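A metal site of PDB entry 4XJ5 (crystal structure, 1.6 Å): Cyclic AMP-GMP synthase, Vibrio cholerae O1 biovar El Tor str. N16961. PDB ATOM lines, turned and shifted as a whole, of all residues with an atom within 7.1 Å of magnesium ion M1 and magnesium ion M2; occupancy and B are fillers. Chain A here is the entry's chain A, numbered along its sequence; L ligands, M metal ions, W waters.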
ATOM      1  N   GLN A 112      -4.232 -25.990 -16.009  1.00  0.00           N
ATOM      2  CA  GLN A 112      -3.279 -24.883 -15.818  1.00  0.00           C
ATOM      3  C   GLN A 112      -1.904 -25.416 -16.155  1.00  0.00           C
ATOM      4  O   GLN A 112      -1.762 -26.590 -16.449  1.00  0.00           O
ATOM      5  CB  GLN A 112      -3.325 -24.359 -14.376  1.00  0.00           C
ATOM      6  CG  GLN A 112      -2.883 -25.384 -13.303  1.00  0.00           C
ATOM      7  CD  GLN A 112      -3.240 -24.954 -11.890  1.00  0.00           C
ATOM      8  OE1 GLN A 112      -4.415 -24.925 -11.547  1.00  0.00           O
ATOM      9  NE2 GLN A 112      -2.236 -24.650 -11.060  1.00  0.00           N
ATOM     10  N   GLY A 113      -0.879 -24.551 -16.185  1.00  0.00           N
ATOM     11  CA  GLY A 113       0.462 -25.085 -16.375  1.00  0.00           C
ATOM     12  C   GLY A 113       0.822 -25.406 -17.818  1.00  0.00           C
ATOM     13  O   GLY A 113       0.148 -24.976 -18.771  1.00  0.00           O
ATOM     14  N   SER A 114       1.875 -26.207 -17.972  1.00  0.00           N
ATOM     15  CA  SER A 114       2.502 -26.387 -19.272  1.00  0.00           C
ATOM     16  C   SER A 114       1.680 -27.148 -20.313  1.00  0.00           C
ATOM     17  O   SER A 114       1.880 -26.975 -21.506  1.00  0.00           O
ATOM     18  CB  SER A 114       3.904 -27.039 -19.086  1.00  0.00           C
ATOM     19  OG  SER A 114       3.854 -28.346 -18.517  1.00  0.00           O
ATOM     20  N   PHE A 115       0.708 -27.959 -19.891  1.00  0.00           N
ATOM     21  CA  PHE A 115      -0.173 -28.524 -20.879  1.00  0.00           C
ATOM     22  C   PHE A 115      -1.114 -27.454 -21.468  1.00  0.00           C
ATOM     23  O   PHE A 115      -1.513 -27.543 -22.638  1.00  0.00           O
ATOM     24  CB  PHE A 115      -0.998 -29.684 -20.273  1.00  0.00           C
ATOM     25  CG  PHE A 115      -1.611 -30.601 -21.308  1.00  0.00           C
ATOM     26  CD1 PHE A 115      -0.833 -31.485 -22.024  1.00  0.00           C
ATOM     27  CD2 PHE A 115      -2.979 -30.602 -21.513  1.00  0.00           C
ATOM     28  CE1 PHE A 115      -1.383 -32.331 -22.967  1.00  0.00           C
ATOM     29  CE2 PHE A 115      -3.548 -31.460 -22.460  1.00  0.00           C
ATOM     30  CZ  PHE A 115      -2.755 -32.332 -23.181  1.00  0.00           C
ATOM     31  N   TYR A 117      -0.447 -23.948 -21.652  1.00  0.00           N
ATOM     32  CA  TYR A 117       0.236 -22.984 -22.509  1.00  0.00           C
ATOM     33  C   TYR A 117       1.412 -23.576 -23.318  1.00  0.00           C
ATOM     34  O   TYR A 117       2.315 -22.849 -23.721  1.00  0.00           O
ATOM     35  CB  TYR A 117       0.723 -21.784 -21.687  1.00  0.00           C
ATOM     36  CG  TYR A 117       1.291 -22.057 -20.301  1.00  0.00           C
ATOM     37  CD1 TYR A 117       2.516 -22.714 -20.124  1.00  0.00           C
ATOM     38  CD2 TYR A 117       0.604 -21.605 -19.167  1.00  0.00           C
ATOM     39  CE1 TYR A 117       3.051 -22.895 -18.843  1.00  0.00           C
ATOM     40  CE2 TYR A 117       1.111 -21.788 -17.896  1.00  0.00           C
ATOM     41  CZ  TYR A 117       2.322 -22.459 -17.715  1.00  0.00           C
ATOM     42  OH  TYR A 117       2.815 -22.632 -16.458  1.00  0.00           O
ATOM     43  N   LEU A 120       5.021 -28.248 -22.374  1.00  0.00           N
ATOM     44  CA  LEU A 120       5.227 -29.536 -21.729  1.00  0.00           C
ATOM     45  C   LEU A 120       6.245 -30.380 -22.525  1.00  0.00           C
ATOM     46  O   LEU A 120       5.984 -30.783 -23.657  1.00  0.00           O
ATOM     47  CB  LEU A 120       3.890 -30.283 -21.621  1.00  0.00           C
ATOM     48  CG  LEU A 120       4.006 -31.680 -20.995  1.00  0.00           C
ATOM     49  CD1 LEU A 120       4.664 -31.620 -19.614  1.00  0.00           C
ATOM     50  CD2 LEU A 120       2.631 -32.339 -20.935  1.00  0.00           C
ATOM     51  N   MET A 130       6.328 -36.538 -17.014  1.00  0.00           N
ATOM     52  CA  MET A 130       5.452 -35.504 -17.538  1.00  0.00           C
ATOM     53  C   MET A 130       4.347 -35.173 -16.543  1.00  0.00           C
ATOM     54  O   MET A 130       3.832 -36.082 -15.908  1.00  0.00           O
ATOM     55  CB  MET A 130       4.800 -35.986 -18.826  1.00  0.00           C
ATOM     56  CG  MET A 130       5.766 -36.152 -19.968  1.00  0.00           C
ATOM     57  SD  MET A 130       4.840 -36.601 -21.416  1.00  0.00           S
ATOM     58  CE  MET A 130       4.608 -38.362 -21.204  1.00  0.00           C
ATOM     59  N   ASP A 131       3.931 -33.921 -16.502  1.00  0.00           N
ATOM     60  CA  ASP A 131       2.985 -33.373 -15.526  1.00  0.00           C
ATOM     61  C   ASP A 131       1.763 -32.759 -16.229  1.00  0.00           C
ATOM     62  O   ASP A 131       1.917 -31.986 -17.163  1.00  0.00           O
ATOM     63  CB  ASP A 131       3.729 -32.330 -14.675  1.00  0.00           C
ATOM     64  CG  ASP A 131       2.864 -31.662 -13.631  1.00  0.00           C
ATOM     65  OD1 ASP A 131       2.154 -32.370 -12.881  1.00  0.00           O
ATOM     66  OD2 ASP A 131       2.893 -30.426 -13.571  1.00  0.00           O
ATOM     67  N   ILE A 132       0.567 -33.102 -15.774  1.00  0.00           N
ATOM     68  CA  ILE A 132      -0.653 -32.443 -16.228  1.00  0.00           C
ATOM     69  C   ILE A 132      -1.292 -31.826 -15.005  1.00  0.00           C
ATOM     70  O   ILE A 132      -1.582 -32.532 -14.056  1.00  0.00           O
ATOM     71  CB  ILE A 132      -1.684 -33.399 -16.838  1.00  0.00           C
ATOM     72  CG1 ILE A 132      -1.075 -34.175 -17.993  1.00  0.00           C
ATOM     73  CG2 ILE A 132      -2.904 -32.598 -17.284  1.00  0.00           C
ATOM     74  CD1 ILE A 132      -0.670 -33.305 -19.114  1.00  0.00           C
ATOM     75  N   ASP A 133      -1.486 -30.506 -15.021  1.00  0.00           N
ATOM     76  CA  ASP A 133      -2.096 -29.813 -13.888  1.00  0.00           C
ATOM     77  C   ASP A 133      -3.552 -29.537 -14.202  1.00  0.00           C
ATOM     78  O   ASP A 133      -3.874 -28.587 -14.897  1.00  0.00           O
ATOM     79  CB  ASP A 133      -1.365 -28.505 -13.624  1.00  0.00           C
ATOM     80  CG  ASP A 133       0.090 -28.702 -13.310  1.00  0.00           C
ATOM     81  OD1 ASP A 133       0.417 -29.044 -12.179  1.00  0.00           O
ATOM     82  OD2 ASP A 133       0.955 -28.433 -14.180  1.00  0.00           O
ATOM     83  N   ASP A 134      -4.465 -30.370 -13.699  1.00  0.00           N
ATOM     84  CA  ASP A 134      -5.860 -30.157 -14.038  1.00  0.00           C
ATOM     85  C   ASP A 134      -6.641 -29.789 -12.786  1.00  0.00           C
ATOM     86  O   ASP A 134      -6.906 -30.628 -11.911  1.00  0.00           O
ATOM     87  CB  ASP A 134      -6.472 -31.384 -14.686  1.00  0.00           C
ATOM     88  CG  ASP A 134      -7.776 -31.053 -15.392  1.00  0.00           C
ATOM     89  OD1 ASP A 134      -7.788 -30.079 -16.167  1.00  0.00           O
ATOM     90  OD2 ASP A 134      -8.808 -31.694 -15.118  1.00  0.00           O
ATOM     91  N   CYS A 180      -2.353 -30.157  -3.855  1.00  0.00           N
ATOM     92  CA  CYS A 180      -3.144 -31.014  -4.725  1.00  0.00           C
ATOM     93  C   CYS A 180      -3.075 -32.478  -4.342  1.00  0.00           C
ATOM     94  O   CYS A 180      -2.215 -32.893  -3.581  1.00  0.00           O
ATOM     95  CB  CYS A 180      -2.682 -30.875  -6.173  1.00  0.00           C
ATOM     96  SG  CYS A 180      -1.007 -31.498  -6.502  1.00  0.00           S
ATOM     97  N   ARG A 182      -2.398 -36.107  -6.302  1.00  0.00           N
ATOM     98  CA  ARG A 182      -1.627 -36.481  -7.473  1.00  0.00           C
ATOM     99  C   ARG A 182      -1.807 -37.955  -7.797  1.00  0.00           C
ATOM    100  O   ARG A 182      -1.765 -38.787  -6.882  1.00  0.00           O
ATOM    101  CB  ARG A 182      -0.166 -36.171  -7.245  1.00  0.00           C
ATOM    102  CG  ARG A 182       0.766 -36.715  -8.336  1.00  0.00           C
ATOM    103  CD  ARG A 182       2.211 -36.281  -8.116  1.00  0.00           C
ATOM    104  NE  ARG A 182       2.390 -34.849  -8.328  1.00  0.00           N
ATOM    105  CZ  ARG A 182       3.568 -34.230  -8.383  1.00  0.00           C
ATOM    106  NH1 ARG A 182       4.696 -34.914  -8.244  1.00  0.00           N
ATOM    107  NH2 ARG A 182       3.619 -32.926  -8.578  1.00  0.00           N
ATOM    108  N   HIS A 191       2.339 -37.992 -14.368  1.00  0.00           N
ATOM    109  CA  HIS A 191       1.456 -37.801 -13.238  1.00  0.00           C
ATOM    110  C   HIS A 191       0.476 -36.658 -13.534  1.00  0.00           C
ATOM    111  O   HIS A 191       0.756 -35.741 -14.327  1.00  0.00           O
ATOM    112  CB  HIS A 191       2.236 -37.565 -11.931  1.00  0.00           C
ATOM    113  CG  HIS A 191       3.153 -36.380 -11.933  1.00  0.00           C
ATOM    114  ND1 HIS A 191       4.525 -36.500 -12.002  1.00  0.00           N
ATOM    115  CD2 HIS A 191       2.896 -35.057 -11.799  1.00  0.00           C
ATOM    116  CE1 HIS A 191       5.074 -35.300 -11.959  1.00  0.00           C
ATOM    117  NE2 HIS A 191       4.101 -34.399 -11.839  1.00  0.00           N
ATOM    118  N   ILE A 192      -0.693 -36.747 -12.901  1.00  0.00           N
ATOM    119  CA  ILE A 192      -1.696 -35.694 -13.011  1.00  0.00           C
ATOM    120  C   ILE A 192      -1.922 -35.122 -11.614  1.00  0.00           C
ATOM    121  O   ILE A 192      -2.150 -35.860 -10.643  1.00  0.00           O
ATOM    122  CB  ILE A 192      -3.016 -36.192 -13.693  1.00  0.00           C
ATOM    123  CG1 ILE A 192      -4.085 -35.092 -13.667  1.00  0.00           C
ATOM    124  CG2 ILE A 192      -3.585 -37.453 -13.039  1.00  0.00           C
ATOM    125  CD1 ILE A 192      -5.201 -35.311 -14.656  1.00  0.00           C
ATOM    126  N   ASP A 193      -1.750 -33.806 -11.530  1.00  0.00           N
ATOM    127  CA  ASP A 193      -2.045 -33.039 -10.318  1.00  0.00           C
ATOM    128  C   ASP A 193      -3.418 -32.437 -10.380  1.00  0.00           C
ATOM    129  O   ASP A 193      -3.834 -31.877 -11.408  1.00  0.00           O
ATOM    130  CB  ASP A 193      -1.031 -31.916 -10.152  1.00  0.00           C
ATOM    131  CG  ASP A 193       0.295 -32.401  -9.621  1.00  0.00           C
ATOM    132  OD1 ASP A 193       0.366 -33.496  -9.032  1.00  0.00           O
ATOM    133  OD2 ASP A 193       1.284 -31.661  -9.806  1.00  0.00           O
ATOM    134  N   VAL A 194      -4.149 -32.535  -9.271  1.00  0.00           N
ATOM    135  CA  VAL A 194      -5.477 -31.955  -9.213  1.00  0.00           C
ATOM    136  C   VAL A 194      -5.561 -30.943  -8.084  1.00  0.00           C
ATOM    137  O   VAL A 194      -5.976 -31.255  -6.958  1.00  0.00           O
ATOM    138  CB  VAL A 194      -6.519 -33.066  -9.055  1.00  0.00           C
ATOM    139  CG1 VAL A 194      -7.937 -32.487  -9.024  1.00  0.00           C
ATOM    140  CG2 VAL A 194      -6.347 -34.059 -10.199  1.00  0.00           C
ATOM    141  N   PRO A 195      -5.152 -29.706  -8.370  1.00  0.00           N
ATOM    142  CA  PRO A 195      -5.390 -28.663  -7.378  1.00  0.00           C
ATOM    143  C   PRO A 195      -6.879 -28.364  -7.309  1.00  0.00           C
ATOM    144  O   PRO A 195      -7.598 -28.526  -8.313  1.00  0.00           O
ATOM    145  CB  PRO A 195      -4.591 -27.462  -7.911  1.00  0.00           C
ATOM    146  CG  PRO A 195      -4.505 -27.693  -9.407  1.00  0.00           C
ATOM    147  CD  PRO A 195      -4.425 -29.214  -9.567  1.00  0.00           C
ATOM    148  N   LYS A 264      13.932 -25.447 -19.571  1.00  0.00           N
ATOM    149  CA  LYS A 264      13.399 -26.580 -18.795  1.00  0.00           C
ATOM    150  C   LYS A 264      14.139 -27.885 -19.121  1.00  0.00           C
ATOM    151  O   LYS A 264      14.391 -28.698 -18.231  1.00  0.00           O
ATOM    152  CB  LYS A 264      11.883 -26.753 -19.034  1.00  0.00           C
ATOM    153  CG  LYS A 264      11.130 -25.595 -18.468  1.00  0.00           C
ATOM    154  CD  LYS A 264       9.681 -25.580 -18.921  1.00  0.00           C
ATOM    155  CE  LYS A 264       8.931 -26.837 -18.473  1.00  0.00           C
ATOM    156  NZ  LYS A 264       7.506 -26.696 -18.930  1.00  0.00           N
ATOM    157  N   SER A 278      10.120 -24.729 -13.000  1.00  0.00           N
ATOM    158  CA  SER A 278       9.767 -24.315 -14.353  1.00  0.00           C
ATOM    159  C   SER A 278       9.282 -22.856 -14.384  1.00  0.00           C
ATOM    160  O   SER A 278       9.692 -22.083 -15.289  1.00  0.00           O
ATOM    161  CB  SER A 278       8.712 -25.257 -14.917  1.00  0.00           C
ATOM    162  OG  SER A 278       9.280 -26.554 -15.076  1.00  0.00           O
HETATM  163  P1  LIG L   1       6.206 -28.333 -15.891  1.00  0.00           P
HETATM  164  O1  LIG L   1       7.540 -28.535 -15.247  1.00  0.00           O
HETATM  165  O2  LIG L   1       6.038 -28.664 -17.342  1.00  0.00           O
HETATM  166  O3  LIG L   1       5.134 -29.043 -15.078  1.00  0.00           O
HETATM  167  O4  LIG L   1       5.841 -26.787 -15.865  1.00  0.00           O
HETATM  168  P2  LIG L   1       4.525 -25.942 -15.477  1.00  0.00           P
HETATM  169  O5  LIG L   1       4.512 -24.678 -16.311  1.00  0.00           O
HETATM  170  O6  LIG L   1       3.297 -26.846 -15.627  1.00  0.00           O
HETATM  171  O7  LIG L   1       4.772 -25.657 -13.946  1.00  0.00           O
HETATM  172  P3  LIG L   1       4.127 -26.291 -12.629  1.00  0.00           P
HETATM  173  O8  LIG L   1       5.139 -26.189 -11.522  1.00  0.00           O
HETATM  174  O9  LIG L   1       3.658 -27.714 -12.861  1.00  0.00           O
HETATM  175  O10 LIG L   1       2.930 -25.290 -12.251  1.00  0.00           O
HETATM  176  C1  LIG L   1       1.728 -25.310 -13.008  1.00  0.00           C
HETATM  177  C2  LIG L   1       0.939 -24.033 -12.696  1.00  0.00           C
HETATM  178  O11 LIG L   1       0.686 -23.959 -11.379  1.00  0.00           O
HETATM  179  C3  LIG L   1       1.732 -22.754 -13.039  1.00  0.00           C
HETATM  180  C4  LIG L   1       1.068 -21.763 -12.062  1.00  0.00           C
HETATM  181  O12 LIG L   1      -0.198 -21.391 -12.712  1.00  0.00           O
HETATM  182  C5  LIG L   1       0.811 -22.453 -10.927  1.00  0.00           C
HETATM  183  N1  LIG L   1       1.934 -22.425 -10.056  1.00  0.00           N
HETATM  184  C6  LIG L   1       2.909 -23.317  -9.767  1.00  0.00           C
HETATM  185  N2  LIG L   1       3.767 -22.749  -8.880  1.00  0.00           N
HETATM  186  C7  LIG L   1       3.300 -21.501  -8.628  1.00  0.00           C
HETATM  187  C8  LIG L   1       3.785 -20.376  -7.761  1.00  0.00           C
HETATM  188  O13 LIG L   1       4.769 -20.479  -7.079  1.00  0.00           O
HETATM  189  N3  LIG L   1       3.047 -19.206  -7.708  1.00  0.00           N
HETATM  190  C9  LIG L   1       1.858 -19.056  -8.469  1.00  0.00           C
HETATM  191  N4  LIG L   1       1.125 -17.865  -8.427  1.00  0.00           N
HETATM  192  N5  LIG L   1       1.408 -20.103  -9.308  1.00  0.00           N
HETATM  193  C10 LIG L   1       2.168 -21.326  -9.356  1.00  0.00           C
HETATM  194  O1  LG2 L   2       4.888 -29.156  -7.592  1.00  0.00           O
HETATM  195  P1  LG2 L   2       4.095 -28.615  -6.333  1.00  0.00           P
HETATM  196  O2  LG2 L   2       4.740 -27.370  -5.785  1.00  0.00           O
HETATM  197  O3  LG2 L   2       4.129 -29.633  -5.231  1.00  0.00           O
HETATM  198  O4  LG2 L   2       2.582 -28.254  -6.720  1.00  0.00           O
HETATM  199  C1  LG2 L   2       1.718 -29.259  -7.246  1.00  0.00           C
HETATM  200  C2  LG2 L   2       0.645 -28.585  -8.129  1.00  0.00           C
HETATM  201  O5  LG2 L   2      -0.119 -27.758  -7.439  1.00  0.00           O
HETATM  202  C3  LG2 L   2       1.278 -27.694  -9.250  1.00  0.00           C
HETATM  203  C4  LG2 L   2       0.101 -26.735  -9.516  1.00  0.00           C
HETATM  204  O6  LG2 L   2      -0.852 -27.517 -10.347  1.00  0.00           O
HETATM  205  C5  LG2 L   2      -0.416 -26.467  -8.318  1.00  0.00           C
HETATM  206  N1  LG2 L   2       0.220 -25.428  -7.597  1.00  0.00           N
HETATM  207  C6  LG2 L   2       1.381 -25.429  -6.858  1.00  0.00           C
HETATM  208  N2  LG2 L   2       1.587 -24.173  -6.366  1.00  0.00           N
HETATM  209  C7  LG2 L   2       0.560 -23.413  -6.794  1.00  0.00           C
HETATM  210  C8  LG2 L   2       0.220 -21.979  -6.574  1.00  0.00           C
HETATM  211  O7  LG2 L   2       0.948 -21.253  -5.915  1.00  0.00           O
HETATM  212  N3  LG2 L   2      -0.948 -21.468  -7.139  1.00  0.00           N
HETATM  213  C9  LG2 L   2      -1.815 -22.281  -7.913  1.00  0.00           C
HETATM  214  N4  LG2 L   2      -2.977 -21.726  -8.508  1.00  0.00           N
HETATM  215  N5  LG2 L   2      -1.474 -23.643  -8.146  1.00  0.00           N
HETATM  216  C10 LG2 L   2      -0.293 -24.195  -7.526  1.00  0.00           C
HETATM  217 MG    MG M   1       1.932 -30.534 -11.464  1.00  0.00          MG
HETATM  218 MG    MG M   2       3.049 -28.744 -14.610  1.00  0.00          MG
HETATM  219  O   HOH W   1       3.767 -29.617 -10.679  1.00  0.00           O
HETATM  220  O   HOH W   2       2.384 -29.293 -16.454  1.00  0.00           O
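An oxygen (O5) of LIG L1 lies within hydrogen-bond range of the side-chain hydroxyl (OH) of Tyr 117 (2.7 Å).
OG of Ser 114 lies within hydrogen-bond range of O2 of LIG L1.
O6 of LG2 L2 lies close to OD1 of Asp 133 (2.7 Å).
An oxygen (O5) of LIG L1 is in hydrogen-bond range of the backbone NH of Ser 114 (3.5 Å).
The side-chain hydroxyl (OG) of Ser 278 is in hydrogen-bond range of an oxygen (O1) of LIG L1 (2.6 Å).
The side-chain amino group (NZ) of Lys 264 is in salt-bridge range of an oxygen (O2) of LIG L1 (2.9 Å).
NE2 of Gln 112 is in hydrogen-bond range of O11 of LIG L1, at 3.0 Å.
NE2 of Gln 112 lies within hydrogen-bond range of N5 of LG2 L2, at 3.2 Å.
A nitrogen (N3) of LIG L1 is in hydrogen-bond range of an oxygen (O7) of LG2 L2, 3.4 Å away.
N of Gln 112 is in hydrogen-bond range of O of Asp 133.
OD1 of Asp 193 sits close to SG of Cys 180 (3.5 Å).
The side-chain carboxylate of Asp 131 lies close to a ring nitrogen (NE2) of His 191 (3.0 Å).
NE of Arg 182 is in salt-bridge range of OD1 of Asp 193, 2.5 Å away.
The backbone NH (N) of Asp 193 is in hydrogen-bond range of the backbone carbonyl oxygen (O) of Ile 132, at 2.8 Å.
The backbone carbonyl oxygen (O) of Asp 193 lies within hydrogen-bond range of the backbone NH (N) of Asp 134.
The nearest printed residue that does not touch magnesium ion M1 is Arg 182 (4.1 Å).
The nearest printed residue that does not touch magnesium ion M2 is Ser 114 (4.01 Å).
Magnesium ion M1 is bound by OD2 of Asp 193 (2.1 Å), water W1 (2.2 Å), OD1 of Asp 133 (2.2 Å), OD2 of Asp 131 (2.3 Å) and OD1 of Asp 131 (2.3 Å).
Magnesium ion M2 is bound by the side-chain carboxylate of Asp 131 (2.0 Å), water W2 (2.0 Å), an oxygen (O9) of LIG L1 (2.1 Å), an oxygen (O3) of LIG L1 (2.2 Å), the side-chain carboxylate of Asp 133 (2.2 Å) and an oxygen (O6) of LIG L1 (2.2 Å).
Magnesium ion M2 has six donor atoms within binding distance.
Water W2 lies within hydrogen-bond range of OG of Ser 114 and O of Asp 131.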
